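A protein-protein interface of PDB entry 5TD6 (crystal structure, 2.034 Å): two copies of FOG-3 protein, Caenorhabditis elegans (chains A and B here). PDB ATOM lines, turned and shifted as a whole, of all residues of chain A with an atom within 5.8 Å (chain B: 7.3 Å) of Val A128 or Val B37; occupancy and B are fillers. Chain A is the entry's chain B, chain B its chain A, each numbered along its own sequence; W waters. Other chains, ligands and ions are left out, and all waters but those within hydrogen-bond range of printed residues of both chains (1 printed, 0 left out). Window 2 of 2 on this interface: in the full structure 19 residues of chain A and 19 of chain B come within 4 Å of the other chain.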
ATOM      1  N   VAL A 124      20.026  17.497 -14.797  1.00  0.00           N
ATOM      2  CA  VAL A 124      19.663  16.087 -14.781  1.00  0.00           C
ATOM      3  C   VAL A 124      20.526  15.328 -15.782  1.00  0.00           C
ATOM      4  O   VAL A 124      20.676  15.778 -16.908  1.00  0.00           O
ATOM      5  CB  VAL A 124      18.173  15.871 -15.123  1.00  0.00           C
ATOM      6  CG1 VAL A 124      17.858  14.393 -15.136  1.00  0.00           C
ATOM      7  CG2 VAL A 124      17.261  16.623 -14.118  1.00  0.00           C
ATOM      8  N   PRO A 125      21.104  14.191 -15.363  1.00  0.00           N
ATOM      9  CA  PRO A 125      21.970  13.373 -16.227  1.00  0.00           C
ATOM     10  C   PRO A 125      21.241  12.868 -17.477  1.00  0.00           C
ATOM     11  O   PRO A 125      20.094  12.407 -17.393  1.00  0.00           O
ATOM     12  CB  PRO A 125      22.362  12.201 -15.333  1.00  0.00           C
ATOM     13  CG  PRO A 125      22.200  12.711 -13.920  1.00  0.00           C
ATOM     14  CD  PRO A 125      21.083  13.706 -13.965  1.00  0.00           C
ATOM     15  N   GLU A 126      21.913  12.944 -18.618  1.00  0.00           N
ATOM     16  CA  GLU A 126      21.298  12.616 -19.906  1.00  0.00           C
ATOM     17  C   GLU A 126      20.526  11.300 -19.923  1.00  0.00           C
ATOM     18  O   GLU A 126      19.404  11.240 -20.450  1.00  0.00           O
ATOM     19  CB  GLU A 126      22.374  12.581 -21.009  1.00  0.00           C
ATOM     20  CG  GLU A 126      21.788  12.036 -22.327  1.00  0.00           C
ATOM     21  CD  GLU A 126      22.802  11.899 -23.421  1.00  0.00           C
ATOM     22  OE1 GLU A 126      23.811  12.626 -23.388  1.00  0.00           O
ATOM     23  OE2 GLU A 126      22.575  11.087 -24.338  1.00  0.00           O
ATOM     24  N   TYR A 127      21.106  10.240 -19.357  1.00  0.00           N
ATOM     25  CA  TYR A 127      20.452   8.933 -19.455  1.00  0.00           C
ATOM     26  C   TYR A 127      19.153   8.872 -18.652  1.00  0.00           C
ATOM     27  O   TYR A 127      18.245   8.137 -19.011  1.00  0.00           O
ATOM     28  CB  TYR A 127      21.360   7.806 -18.992  1.00  0.00           C
ATOM     29  CG  TYR A 127      20.943   6.476 -19.559  1.00  0.00           C
ATOM     30  CD1 TYR A 127      21.110   6.209 -20.906  1.00  0.00           C
ATOM     31  CD2 TYR A 127      20.360   5.498 -18.763  1.00  0.00           C
ATOM     32  CE1 TYR A 127      20.735   4.999 -21.452  1.00  0.00           C
ATOM     33  CE2 TYR A 127      19.977   4.275 -19.302  1.00  0.00           C
ATOM     34  CZ  TYR A 127      20.168   4.034 -20.646  1.00  0.00           C
ATOM     35  OH  TYR A 127      19.799   2.825 -21.208  1.00  0.00           O
ATOM     36  N   VAL A 128      19.100   9.612 -17.553  1.00  0.00           N
ATOM     37  CA  VAL A 128      17.875   9.733 -16.754  1.00  0.00           C
ATOM     38  C   VAL A 128      16.807  10.407 -17.601  1.00  0.00           C
ATOM     39  O   VAL A 128      15.671   9.942 -17.675  1.00  0.00           O
ATOM     40  CB  VAL A 128      18.125  10.542 -15.445  1.00  0.00           C
ATOM     41  CG1 VAL A 128      16.815  10.916 -14.739  1.00  0.00           C
ATOM     42  CG2 VAL A 128      19.056   9.773 -14.533  1.00  0.00           C
ATOM     43  N   VAL A 129      17.200  11.479 -18.286  1.00  0.00           N
ATOM     44  CA  VAL A 129      16.287  12.216 -19.148  1.00  0.00           C
ATOM     45  C   VAL A 129      15.785  11.341 -20.300  1.00  0.00           C
ATOM     46  O   VAL A 129      14.595  11.341 -20.590  1.00  0.00           O
ATOM     47  CB  VAL A 129      16.945  13.511 -19.698  1.00  0.00           C
ATOM     48  CG1 VAL A 129      16.031  14.189 -20.683  1.00  0.00           C
ATOM     49  CG2 VAL A 129      17.254  14.459 -18.560  1.00  0.00           C
ATOM     50  N   ARG A 130      16.669  10.584 -20.953  1.00  0.00           N
ATOM     51  CA  ARG A 130      16.220   9.695 -22.023  1.00  0.00           C
ATOM     52  C   ARG A 130      15.311   8.615 -21.456  1.00  0.00           C
ATOM     53  O   ARG A 130      14.348   8.200 -22.094  1.00  0.00           O
ATOM     54  CB  ARG A 130      17.398   9.025 -22.748  1.00  0.00           C
ATOM     55  CG  ARG A 130      18.216   9.979 -23.552  1.00  0.00           C
ATOM     56  CD  ARG A 130      19.215   9.271 -24.439  1.00  0.00           C
ATOM     57  NE  ARG A 130      20.061  10.299 -25.022  1.00  0.00           N
ATOM     58  CZ  ARG A 130      19.874  10.851 -26.212  1.00  0.00           C
ATOM     59  NH1 ARG A 130      18.900  10.419 -27.018  1.00  0.00           N
ATOM     60  NH2 ARG A 130      20.720  11.805 -26.618  1.00  0.00           N
ATOM     61  N   THR A 131      15.641   8.149 -20.260  1.00  0.00           N
ATOM     62  CA  THR A 131      14.915   7.031 -19.672  1.00  0.00           C
ATOM     63  C   THR A 131      13.476   7.457 -19.391  1.00  0.00           C
ATOM     64  O   THR A 131      12.530   6.742 -19.728  1.00  0.00           O
ATOM     65  CB  THR A 131      15.612   6.531 -18.405  1.00  0.00           C
ATOM     66  OG1 THR A 131      16.785   5.790 -18.782  1.00  0.00           O
ATOM     67  CG2 THR A 131      14.679   5.640 -17.583  1.00  0.00           C
ATOM     68  N   ALA A 132      13.324   8.650 -18.827  1.00  0.00           N
ATOM     69  CA  ALA A 132      12.007   9.213 -18.553  1.00  0.00           C
ATOM     70  C   ALA A 132      11.236   9.408 -19.842  1.00  0.00           C
ATOM     71  O   ALA A 132      10.090   8.976 -19.963  1.00  0.00           O
ATOM     72  CB  ALA A 132      12.134  10.530 -17.815  1.00  0.00           C
ATOM     73  N   ALA A 133      11.888  10.049 -20.807  1.00  0.00           N
ATOM     74  CA  ALA A 133      11.278  10.384 -22.084  1.00  0.00           C
ATOM     75  C   ALA A 133      10.698   9.153 -22.752  1.00  0.00           C
ATOM     76  O   ALA A 133       9.558   9.161 -23.221  1.00  0.00           O
ATOM     77  CB  ALA A 133      12.299  11.048 -23.001  1.00  0.00           C
ATOM     78  N   MET B   1       8.485  11.174 -11.520  1.00  0.00           N
ATOM     79  CA  MET B   1       9.807  11.050 -10.907  1.00  0.00           C
ATOM     80  C   MET B   1      10.364  12.396 -10.442  1.00  0.00           C
ATOM     81  O   MET B   1      10.728  12.546  -9.277  1.00  0.00           O
ATOM     82  CB  MET B   1      10.800  10.400 -11.869  1.00  0.00           C
ATOM     83  CG  MET B   1      12.255  10.656 -11.480  1.00  0.00           C
ATOM     84  SD  MET B   1      12.804   9.714 -10.041  1.00  0.00           S
ATOM     85  CE  MET B   1      13.003   8.114 -10.810  1.00  0.00           C
ATOM     86  N   TYR B   2      10.446  13.368 -11.348  1.00  0.00           N
ATOM     87  CA  TYR B   2      10.979  14.680 -10.987  1.00  0.00           C
ATOM     88  C   TYR B   2      10.123  15.345  -9.901  1.00  0.00           C
ATOM     89  O   TYR B   2      10.636  15.972  -8.977  1.00  0.00           O
ATOM     90  CB  TYR B   2      11.031  15.600 -12.200  1.00  0.00           C
ATOM     91  CG  TYR B   2      11.871  15.100 -13.350  1.00  0.00           C
ATOM     92  CD1 TYR B   2      13.150  14.592 -13.145  1.00  0.00           C
ATOM     93  CD2 TYR B   2      11.374  15.131 -14.642  1.00  0.00           C
ATOM     94  CE1 TYR B   2      13.934  14.144 -14.231  1.00  0.00           C
ATOM     95  CE2 TYR B   2      12.120  14.680 -15.708  1.00  0.00           C
ATOM     96  CZ  TYR B   2      13.395  14.192 -15.503  1.00  0.00           C
ATOM     97  OH  TYR B   2      14.112  13.751 -16.584  1.00  0.00           O
ATOM     98  N   VAL B   5      10.696  13.705  -6.463  1.00  0.00           N
ATOM     99  CA  VAL B   5      12.016  14.043  -5.923  1.00  0.00           C
ATOM    100  C   VAL B   5      12.073  15.499  -5.441  1.00  0.00           C
ATOM    101  O   VAL B   5      12.600  15.799  -4.364  1.00  0.00           O
ATOM    102  CB  VAL B   5      13.129  13.794  -6.980  1.00  0.00           C
ATOM    103  CG1 VAL B   5      14.404  14.595  -6.654  1.00  0.00           C
ATOM    104  CG2 VAL B   5      13.434  12.314  -7.087  1.00  0.00           C
ATOM    105  N   ALA B  30      19.816  20.790  -4.636  1.00  0.00           N
ATOM    106  CA  ALA B  30      20.074  20.391  -6.017  1.00  0.00           C
ATOM    107  C   ALA B  30      20.843  19.078  -6.046  1.00  0.00           C
ATOM    108  O   ALA B  30      20.456  18.130  -6.725  1.00  0.00           O
ATOM    109  CB  ALA B  30      20.850  21.482  -6.754  1.00  0.00           C
ATOM    110  N   GLU B  31      21.913  19.016  -5.266  1.00  0.00           N
ATOM    111  CA  GLU B  31      22.737  17.822  -5.208  1.00  0.00           C
ATOM    112  C   GLU B  31      21.987  16.635  -4.610  1.00  0.00           C
ATOM    113  O   GLU B  31      22.159  15.500  -5.060  1.00  0.00           O
ATOM    114  CB  GLU B  31      24.006  18.098  -4.402  1.00  0.00           C
ATOM    115  CG  GLU B  31      25.021  18.940  -5.145  1.00  0.00           C
ATOM    116  CD  GLU B  31      25.427  18.293  -6.455  1.00  0.00           C
ATOM    117  OE1 GLU B  31      25.981  17.167  -6.419  1.00  0.00           O
ATOM    118  OE2 GLU B  31      25.159  18.898  -7.514  1.00  0.00           O
ATOM    119  N   LEU B  32      21.154  16.885  -3.602  1.00  0.00           N
ATOM    120  CA  LEU B  32      20.339  15.811  -3.025  1.00  0.00           C
ATOM    121  C   LEU B  32      19.388  15.245  -4.088  1.00  0.00           C
ATOM    122  O   LEU B  32      19.271  14.015  -4.252  1.00  0.00           O
ATOM    123  CB  LEU B  32      19.550  16.316  -1.797  1.00  0.00           C
ATOM    124  CG  LEU B  32      18.595  15.322  -1.127  1.00  0.00           C
ATOM    125  CD1 LEU B  32      19.319  14.096  -0.554  1.00  0.00           C
ATOM    126  CD2 LEU B  32      17.790  16.034  -0.038  1.00  0.00           C
ATOM    127  N   GLY B  33      18.718  16.131  -4.809  1.00  0.00           N
ATOM    128  CA  GLY B  33      17.771  15.703  -5.828  1.00  0.00           C
ATOM    129  C   GLY B  33      18.460  14.917  -6.934  1.00  0.00           C
ATOM    130  O   GLY B  33      17.910  13.947  -7.482  1.00  0.00           O
ATOM    131  N   ASN B  34      19.678  15.320  -7.261  1.00  0.00           N
ATOM    132  CA  ASN B  34      20.421  14.619  -8.306  1.00  0.00           C
ATOM    133  C   ASN B  34      20.787  13.225  -7.844  1.00  0.00           C
ATOM    134  O   ASN B  34      20.653  12.263  -8.591  1.00  0.00           O
ATOM    135  CB  ASN B  34      21.689  15.379  -8.719  1.00  0.00           C
ATOM    136  CG  ASN B  34      22.473  14.619  -9.771  1.00  0.00           C
ATOM    137  OD1 ASN B  34      22.065  14.557 -10.937  1.00  0.00           O
ATOM    138  ND2 ASN B  34      23.566  13.987  -9.357  1.00  0.00           N
ATOM    139  N   TYR B  35      21.232  13.105  -6.599  1.00  0.00           N
ATOM    140  CA  TYR B  35      21.456  11.786  -6.041  1.00  0.00           C
ATOM    141  C   TYR B  35      20.193  10.932  -6.090  1.00  0.00           C
ATOM    142  O   TYR B  35      20.231   9.759  -6.485  1.00  0.00           O
ATOM    143  CB  TYR B  35      21.944  11.881  -4.604  1.00  0.00           C
ATOM    144  CG  TYR B  35      21.900  10.558  -3.895  1.00  0.00           C
ATOM    145  CD1 TYR B  35      22.833   9.565  -4.174  1.00  0.00           C
ATOM    146  CD2 TYR B  35      20.925  10.288  -2.947  1.00  0.00           C
ATOM    147  CE1 TYR B  35      22.794   8.342  -3.527  1.00  0.00           C
ATOM    148  CE2 TYR B  35      20.880   9.071  -2.294  1.00  0.00           C
ATOM    149  CZ  TYR B  35      21.821   8.106  -2.585  1.00  0.00           C
ATOM    150  OH  TYR B  35      21.774   6.894  -1.933  1.00  0.00           O
ATOM    151  N   LEU B  36      19.076  11.522  -5.683  1.00  0.00           N
ATOM    152  CA  LEU B  36      17.831  10.780  -5.569  1.00  0.00           C
ATOM    153  C   LEU B  36      17.286  10.376  -6.934  1.00  0.00           C
ATOM    154  O   LEU B  36      16.809   9.256  -7.101  1.00  0.00           O
ATOM    155  CB  LEU B  36      16.779  11.598  -4.810  1.00  0.00           C
ATOM    156  CG  LEU B  36      17.147  11.852  -3.342  1.00  0.00           C
ATOM    157  CD1 LEU B  36      16.125  12.745  -2.672  1.00  0.00           C
ATOM    158  CD2 LEU B  36      17.283  10.533  -2.591  1.00  0.00           C
ATOM    159  N   VAL B  37      17.340  11.284  -7.904  1.00  0.00           N
ATOM    160  CA  VAL B  37      16.739  10.987  -9.198  1.00  0.00           C
ATOM    161  C   VAL B  37      17.493   9.838  -9.876  1.00  0.00           C
ATOM    162  O   VAL B  37      16.895   9.044 -10.600  1.00  0.00           O
ATOM    163  CB  VAL B  37      16.686  12.232 -10.112  1.00  0.00           C
ATOM    164  CG1 VAL B  37      18.053  12.540 -10.715  1.00  0.00           C
ATOM    165  CG2 VAL B  37      15.660  12.026 -11.213  1.00  0.00           C
ATOM    166  N   SER B  38      18.786   9.709  -9.588  1.00  0.00           N
ATOM    167  CA  SER B  38      19.588   8.621 -10.140  1.00  0.00           C
ATOM    168  C   SER B  38      19.391   7.328  -9.346  1.00  0.00           C
ATOM    169  O   SER B  38      19.295   6.243  -9.919  1.00  0.00           O
ATOM    170  CB  SER B  38      21.071   9.006 -10.162  1.00  0.00           C
ATOM    171  OG  SER B  38      21.289  10.200 -10.898  1.00  0.00           O
ATOM    172  N   HIS B  39      19.323   7.461  -8.027  1.00  0.00           N
ATOM    173  CA  HIS B  39      19.150   6.339  -7.104  1.00  0.00           C
ATOM    174  C   HIS B  39      17.733   5.751  -7.187  1.00  0.00           C
ATOM    175  O   HIS B  39      17.487   4.625  -6.751  1.00  0.00           O
ATOM    176  CB  HIS B  39      19.479   6.817  -5.684  1.00  0.00           C
ATOM    177  CG  HIS B  39      19.153   5.844  -4.590  1.00  0.00           C
ATOM    178  ND1 HIS B  39      20.037   4.874  -4.165  1.00  0.00           N
ATOM    179  CD2 HIS B  39      18.067   5.736  -3.787  1.00  0.00           C
ATOM    180  CE1 HIS B  39      19.496   4.191  -3.173  1.00  0.00           C
ATOM    181  NE2 HIS B  39      18.301   4.695  -2.921  1.00  0.00           N
ATOM    182  N   PHE B  40      16.811   6.521  -7.763  1.00  0.00           N
ATOM    183  CA  PHE B  40      15.417   6.109  -7.881  1.00  0.00           C
ATOM    184  C   PHE B  40      15.125   5.497  -9.245  1.00  0.00           C
ATOM    185  O   PHE B  40      14.233   4.672  -9.367  1.00  0.00           O
ATOM    186  CB  PHE B  40      14.457   7.296  -7.674  1.00  0.00           C
ATOM    187  CG  PHE B  40      14.332   7.783  -6.237  1.00  0.00           C
ATOM    188  CD1 PHE B  40      14.951   7.127  -5.187  1.00  0.00           C
ATOM    189  CD2 PHE B  40      13.556   8.901  -5.951  1.00  0.00           C
ATOM    190  CE1 PHE B  40      14.814   7.599  -3.882  1.00  0.00           C
ATOM    191  CE2 PHE B  40      13.416   9.372  -4.648  1.00  0.00           C
ATOM    192  CZ  PHE B  40      14.046   8.730  -3.620  1.00  0.00           C
ATOM    193  N   SER B  41      15.864   5.929 -10.265  1.00  0.00           N
ATOM    194  CA  SER B  41      15.512   5.654 -11.662  1.00  0.00           C
ATOM    195  C   SER B  41      15.403   4.164 -11.983  1.00  0.00           C
ATOM    196  O   SER B  41      14.514   3.748 -12.731  1.00  0.00           O
ATOM    197  CB  SER B  41      16.525   6.311 -12.605  1.00  0.00           C
ATOM    198  OG  SER B  41      15.964   6.514 -13.897  1.00  0.00           O
ATOM    199  N   SER B  42      16.283   3.367 -11.388  1.00  0.00           N
ATOM    200  CA  SER B  42      16.321   1.936 -11.653  1.00  0.00           C
ATOM    201  C   SER B  42      15.040   1.191 -11.251  1.00  0.00           C
ATOM    202  O   SER B  42      14.752   0.130 -11.808  1.00  0.00           O
ATOM    203  CB  SER B  42      17.528   1.310 -10.945  1.00  0.00           C
ATOM    204  OG  SER B  42      17.624   1.756  -9.604  1.00  0.00           O
ATOM    205  N   TRP B  44      11.841   3.012 -10.554  1.00  0.00           N
ATOM    206  CA  TRP B  44      10.630   3.806 -10.754  1.00  0.00           C
ATOM    207  C   TRP B  44       9.691   3.167 -11.784  1.00  0.00           C
ATOM    208  O   TRP B  44       9.924   3.232 -12.993  1.00  0.00           O
ATOM    209  CB  TRP B  44      10.979   5.226 -11.188  1.00  0.00           C
ATOM    210  CG  TRP B  44      10.003   6.264 -10.707  1.00  0.00           C
ATOM    211  CD1 TRP B  44       9.035   6.887 -11.438  1.00  0.00           C
ATOM    212  CD2 TRP B  44       9.920   6.805  -9.384  1.00  0.00           C
ATOM    213  NE1 TRP B  44       8.352   7.786 -10.653  1.00  0.00           N
ATOM    214  CE2 TRP B  44       8.877   7.751  -9.386  1.00  0.00           C
ATOM    215  CE3 TRP B  44      10.623   6.573  -8.197  1.00  0.00           C
ATOM    216  CZ2 TRP B  44       8.520   8.464  -8.246  1.00  0.00           C
ATOM    217  CZ3 TRP B  44      10.266   7.287  -7.060  1.00  0.00           C
ATOM    218  CH2 TRP B  44       9.233   8.221  -7.096  1.00  0.00           C
HETATM  219  O   HOH W   1      14.472   8.467 -15.547  1.00  0.00           O
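O of Asn B34 is in hydrogen-bond range of OG of Ser B38 (3.2 Å).
Among the printed residues, pairs that only touch across the chains: Pro A125 with Asn B34, Val A129 with Tyr B2, Val A128 with Val B37 and Ala A132 with Tyr B2.
Val A128 touches just one residue of chain B: Val B37 (3.9 Å).
Val B37 touches just one residue of chain A: Val A128 (3.9 Å).
Of the printed residues of chain A, Tyr B2 touches Val A129 (3.7 Å) and Ala A132 (3.98 Å).
Of the printed residues of chain B, Val A129 touches Tyr B2.
Printed residues of chain A within 4 Å of Asn B34: Pro A125 (3.3 Å).
Of the printed residues of chain B, Ala A132 touches Tyr B2 (3.98 Å).
Of the printed residues of chain B, Pro A125 touches Asn B34 (3.3 Å).
Leu B36 touches none of the printed residues of chain A.
Arg A130 touches none of the printed residues of chain B.
The nearest printed residue of chain B that does not touch Pro A125 is Ser B38 (4.03 Å).
Of the 17 printed residues of chain B, 3 touch a printed residue of chain A.
Hydrophobic or aromatic side chains of chain B within 4 Å of the printed part of chain A: Tyr B2 and Val B37.
Of the 10 printed residues of chain A, 4 touch a printed residue of chain B.
Hydrophobic or aromatic side chains of chain A within 4 Å of the printed part of chain B: Pro A125, Val A128, Val A129 and Ala A132.
Among the printed residues, 4 pairs touch across the chains.
Among the printed residues, no Asp or Glu carboxylate lies within 4 Å of a Lys or Arg side-chain nitrogen of the other chain.
No position is printed for both chains.
Water W1 lies within hydrogen-bond range of the backbone carbonyl oxygen (O) of Val A128 (2.9 Å), the side-chain hydroxyl (OG) of Ser B41 (3.0 Å) and the backbone NH (N) of Ala A132 (3.5 Å).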
